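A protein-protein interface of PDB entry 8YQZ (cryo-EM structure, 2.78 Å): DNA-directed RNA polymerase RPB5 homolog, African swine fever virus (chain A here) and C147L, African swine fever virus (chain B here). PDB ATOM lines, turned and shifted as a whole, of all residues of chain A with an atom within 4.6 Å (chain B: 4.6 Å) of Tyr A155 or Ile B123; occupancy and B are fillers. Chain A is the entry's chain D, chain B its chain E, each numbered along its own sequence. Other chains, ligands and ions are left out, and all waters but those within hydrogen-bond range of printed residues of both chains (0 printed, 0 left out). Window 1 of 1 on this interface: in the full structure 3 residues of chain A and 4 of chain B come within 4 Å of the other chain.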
ATOM      1  N   LEU A 151      -6.540  18.421  28.246  1.00  0.00           N
ATOM      2  CA  LEU A 151      -5.297  17.702  28.496  1.00  0.00           C
ATOM      3  C   LEU A 151      -4.546  17.412  27.206  1.00  0.00           C
ATOM      4  O   LEU A 151      -3.315  17.365  27.199  1.00  0.00           O
ATOM      5  CB  LEU A 151      -5.579  16.402  29.238  1.00  0.00           C
ATOM      6  CG  LEU A 151      -6.167  16.470  30.640  1.00  0.00           C
ATOM      7  CD1 LEU A 151      -6.623  15.100  31.060  1.00  0.00           C
ATOM      8  CD2 LEU A 151      -5.179  17.027  31.624  1.00  0.00           C
ATOM      9  N   GLY A 152      -5.265  17.183  26.113  1.00  0.00           N
ATOM     10  CA  GLY A 152      -4.605  16.963  24.843  1.00  0.00           C
ATOM     11  C   GLY A 152      -3.917  18.202  24.315  1.00  0.00           C
ATOM     12  O   GLY A 152      -2.816  18.123  23.767  1.00  0.00           O
ATOM     13  N   ARG A 153      -4.555  19.361  24.454  1.00  0.00           N
ATOM     14  CA  ARG A 153      -3.883  20.596  24.067  1.00  0.00           C
ATOM     15  C   ARG A 153      -2.687  20.880  24.966  1.00  0.00           C
ATOM     16  O   ARG A 153      -1.687  21.440  24.514  1.00  0.00           O
ATOM     17  CB  ARG A 153      -4.867  21.759  24.095  1.00  0.00           C
ATOM     18  CG  ARG A 153      -4.364  23.033  23.467  1.00  0.00           C
ATOM     19  CD  ARG A 153      -3.997  24.059  24.509  1.00  0.00           C
ATOM     20  NE  ARG A 153      -3.403  25.246  23.910  1.00  0.00           N
ATOM     21  CZ  ARG A 153      -2.632  26.105  24.560  1.00  0.00           C
ATOM     22  NH1 ARG A 153      -2.341  25.942  25.835  1.00  0.00           N
ATOM     23  NH2 ARG A 153      -2.148  27.156  23.915  1.00  0.00           N
ATOM     24  N   GLU A 154      -2.767  20.504  26.235  1.00  0.00           N
ATOM     25  CA  GLU A 154      -1.737  20.836  27.204  1.00  0.00           C
ATOM     26  C   GLU A 154      -0.656  19.774  27.339  1.00  0.00           C
ATOM     27  O   GLU A 154       0.310  20.002  28.067  1.00  0.00           O
ATOM     28  CB  GLU A 154      -2.375  21.074  28.570  1.00  0.00           C
ATOM     29  CG  GLU A 154      -3.332  22.229  28.593  1.00  0.00           C
ATOM     30  CD  GLU A 154      -2.655  23.550  28.825  1.00  0.00           C
ATOM     31  OE1 GLU A 154      -1.818  23.649  29.742  1.00  0.00           O
ATOM     32  OE2 GLU A 154      -2.965  24.498  28.083  1.00  0.00           O
ATOM     33  N   TYR A 155      -0.793  18.634  26.666  1.00  0.00           N
ATOM     34  CA  TYR A 155       0.163  17.526  26.748  1.00  0.00           C
ATOM     35  C   TYR A 155       0.347  17.054  28.189  1.00  0.00           C
ATOM     36  O   TYR A 155       1.462  16.929  28.689  1.00  0.00           O
ATOM     37  CB  TYR A 155       1.509  17.906  26.133  1.00  0.00           C
ATOM     38  CG  TYR A 155       1.603  17.692  24.650  1.00  0.00           C
ATOM     39  CD1 TYR A 155       1.762  16.427  24.124  1.00  0.00           C
ATOM     40  CD2 TYR A 155       1.544  18.753  23.775  1.00  0.00           C
ATOM     41  CE1 TYR A 155       1.847  16.226  22.771  1.00  0.00           C
ATOM     42  CE2 TYR A 155       1.631  18.560  22.422  1.00  0.00           C
ATOM     43  CZ  TYR A 155       1.783  17.296  21.926  1.00  0.00           C
ATOM     44  OH  TYR A 155       1.868  17.111  20.572  1.00  0.00           O
ATOM     45  N   LEU A 156      -0.769  16.774  28.852  1.00  0.00           N
ATOM     46  CA  LEU A 156      -0.784  16.406  30.257  1.00  0.00           C
ATOM     47  C   LEU A 156      -1.542  15.103  30.453  1.00  0.00           C
ATOM     48  O   LEU A 156      -2.373  14.714  29.631  1.00  0.00           O
ATOM     49  CB  LEU A 156      -1.433  17.498  31.109  1.00  0.00           C
ATOM     50  CG  LEU A 156      -0.661  18.778  31.411  1.00  0.00           C
ATOM     51  CD1 LEU A 156      -1.576  19.786  32.050  1.00  0.00           C
ATOM     52  CD2 LEU A 156       0.503  18.502  32.310  1.00  0.00           C
ATOM     53  N   GLN A 157      -1.244  14.451  31.507  1.00  0.00           N
ATOM     54  CA  GLN A 157      -1.947  13.318  32.075  1.00  0.00           C
ATOM     55  C   GLN A 157      -2.811  13.772  33.242  1.00  0.00           C
ATOM     56  O   GLN A 157      -2.521  14.791  33.868  1.00  0.00           O
ATOM     57  CB  GLN A 157      -0.963  12.248  32.558  1.00  0.00           C
ATOM     58  CG  GLN A 157      -0.019  11.727  31.494  1.00  0.00           C
ATOM     59  CD  GLN A 157      -0.739  11.279  30.248  1.00  0.00           C
ATOM     60  OE1 GLN A 157      -1.778  10.632  30.316  1.00  0.00           O
ATOM     61  NE2 GLN A 157      -0.199  11.637  29.095  1.00  0.00           N
ATOM     62  N   ILE B  60       6.992  18.625  16.107  1.00  0.00           N
ATOM     63  CA  ILE B  60       5.679  19.233  15.885  1.00  0.00           C
ATOM     64  C   ILE B  60       5.719  20.059  14.607  1.00  0.00           C
ATOM     65  O   ILE B  60       6.663  20.845  14.411  1.00  0.00           O
ATOM     66  CB  ILE B  60       5.284  20.096  17.095  1.00  0.00           C
ATOM     67  CG1 ILE B  60       5.129  19.215  18.327  1.00  0.00           C
ATOM     68  CG2 ILE B  60       4.016  20.853  16.830  1.00  0.00           C
ATOM     69  CD1 ILE B  60       4.924  19.976  19.588  1.00  0.00           C
ATOM     70  N   ARG B 121      12.866  22.967  21.709  1.00  0.00           N
ATOM     71  CA  ARG B 121      12.043  23.073  22.904  1.00  0.00           C
ATOM     72  C   ARG B 121      11.345  21.737  23.105  1.00  0.00           C
ATOM     73  O   ARG B 121      10.473  21.368  22.322  1.00  0.00           O
ATOM     74  CB  ARG B 121      11.040  24.216  22.764  1.00  0.00           C
ATOM     75  CG  ARG B 121      11.665  25.592  22.794  1.00  0.00           C
ATOM     76  CD  ARG B 121      10.654  26.648  22.470  1.00  0.00           C
ATOM     77  NE  ARG B 121      11.147  27.998  22.699  1.00  0.00           N
ATOM     78  CZ  ARG B 121      10.581  29.091  22.214  1.00  0.00           C
ATOM     79  NH1 ARG B 121       9.502  29.033  21.468  1.00  0.00           N
ATOM     80  NH2 ARG B 121      11.121  30.272  22.477  1.00  0.00           N
ATOM     81  N   CYS B 122      11.742  21.004  24.135  1.00  0.00           N
ATOM     82  CA  CYS B 122      11.201  19.676  24.381  1.00  0.00           C
ATOM     83  C   CYS B 122       9.887  19.797  25.134  1.00  0.00           C
ATOM     84  O   CYS B 122       9.857  20.259  26.275  1.00  0.00           O
ATOM     85  CB  CYS B 122      12.189  18.821  25.162  1.00  0.00           C
ATOM     86  SG  CYS B 122      11.556  17.175  25.563  1.00  0.00           S
ATOM     87  N   ILE B 123       8.803  19.342  24.515  1.00  0.00           N
ATOM     88  CA  ILE B 123       7.492  19.486  25.125  1.00  0.00           C
ATOM     89  C   ILE B 123       7.190  18.313  26.047  1.00  0.00           C
ATOM     90  O   ILE B 123       6.865  18.503  27.222  1.00  0.00           O
ATOM     91  CB  ILE B 123       6.418  19.655  24.036  1.00  0.00           C
ATOM     92  CG1 ILE B 123       6.763  20.841  23.136  1.00  0.00           C
ATOM     93  CG2 ILE B 123       5.057  19.823  24.650  1.00  0.00           C
ATOM     94  CD1 ILE B 123       7.054  22.110  23.870  1.00  0.00           C
ATOM     95  N   LYS B 124       7.315  17.087  25.549  1.00  0.00           N
ATOM     96  CA  LYS B 124       6.945  15.923  26.338  1.00  0.00           C
ATOM     97  C   LYS B 124       7.794  14.725  25.938  1.00  0.00           C
ATOM     98  O   LYS B 124       8.272  14.630  24.810  1.00  0.00           O
ATOM     99  CB  LYS B 124       5.460  15.589  26.168  1.00  0.00           C
ATOM    100  CG  LYS B 124       4.922  14.704  27.255  1.00  0.00           C
ATOM    101  CD  LYS B 124       3.529  14.252  26.966  1.00  0.00           C
ATOM    102  CE  LYS B 124       3.044  13.295  28.035  1.00  0.00           C
ATOM    103  NZ  LYS B 124       3.156  13.863  29.401  1.00  0.00           N
ATOM    104  N   ILE B 132       8.647  14.608  21.875  1.00  0.00           N
ATOM    105  CA  ILE B 132       7.924  15.596  21.085  1.00  0.00           C
ATOM    106  C   ILE B 132       8.575  16.954  21.305  1.00  0.00           C
ATOM    107  O   ILE B 132       8.670  17.427  22.439  1.00  0.00           O
ATOM    108  CB  ILE B 132       6.436  15.616  21.461  1.00  0.00           C
ATOM    109  CG1 ILE B 132       5.749  14.343  20.982  1.00  0.00           C
ATOM    110  CG2 ILE B 132       5.743  16.767  20.817  1.00  0.00           C
ATOM    111  CD1 ILE B 132       5.361  13.427  22.075  1.00  0.00           C
ATOM    112  N   VAL B 133       9.046  17.576  20.225  1.00  0.00           N
ATOM    113  CA  VAL B 133       9.816  18.808  20.318  1.00  0.00           C
ATOM    114  C   VAL B 133       9.303  19.823  19.311  1.00  0.00           C
ATOM    115  O   VAL B 133       8.663  19.484  18.317  1.00  0.00           O
ATOM    116  CB  VAL B 133      11.333  18.584  20.103  1.00  0.00           C
ATOM    117  CG1 VAL B 133      11.888  17.611  21.119  1.00  0.00           C
ATOM    118  CG2 VAL B 133      11.613  18.116  18.700  1.00  0.00           C
ATOM    119  N   GLU B 134       9.600  21.086  19.592  1.00  0.00           N
ATOM    120  CA  GLU B 134       9.367  22.199  18.684  1.00  0.00           C
ATOM    121  C   GLU B 134      10.713  22.786  18.294  1.00  0.00           C
ATOM    122  O   GLU B 134      11.526  23.097  19.165  1.00  0.00           O
ATOM    123  CB  GLU B 134       8.515  23.276  19.340  1.00  0.00           C
ATOM    124  CG  GLU B 134       7.037  23.057  19.251  1.00  0.00           C
ATOM    125  CD  GLU B 134       6.271  24.056  20.077  1.00  0.00           C
ATOM    126  OE1 GLU B 134       6.895  25.018  20.549  1.00  0.00           O
ATOM    127  OE2 GLU B 134       5.052  23.889  20.262  1.00  0.00           O
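Ile B123 touches Tyr A155. NZ of Lys B124 touches O of Tyr A155, at 3.6 Å. CG2 of Ile B132 touches OH of Tyr A155, at 3.9 Å. Gln A157 touches Lys B124 (NE2 to CE, 3.8 Å).
The backbone NH (N) of Ile B123 is in hydrogen-bond range of the backbone carbonyl oxygen (O) of Ile B132, 2.8 Å away. The backbone carbonyl oxygen of Lys B124 sits at hydrogen-bond distance from the backbone NH of Ile B132 (3.0 Å).
Along chain B the printed residues that touch a printed residue of chain A span positions 123 to 132. Hydrophobic or aromatic side chains of chain A that line the printed part of chain B: Tyr A155. Among the printed residues, no Asp or Glu carboxylate lies within 4 Å of a Lys or Arg side-chain nitrogen of the other chain.
Of chain B, only Ile B123 (3.8 Å), Lys B124 (3.6 Å) and Ile B132 (3.9 Å) come within 4 Å of Tyr A155. Ile B123 touches just one residue of chain A: Tyr A155 (3.8 Å). Printed residues of chain B within 4 Å of Gln A157: Lys B124. Of the printed residues of chain A, Ile B132 touches Tyr A155. Of the printed residues of chain A, Lys B124 touches Tyr A155 and Gln A157. Leu A151 touches none of the printed residues of chain B. The nearest residue of chain B that does not touch Tyr A155 is Ile B60 (4.3 Å). The nearest printed residue of chain A that does not touch Ile B123 is Glu A154 (5.9 Å). The nearest printed residue of chain B that does not touch Gln A157 is Ile B132 (9.1 Å).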
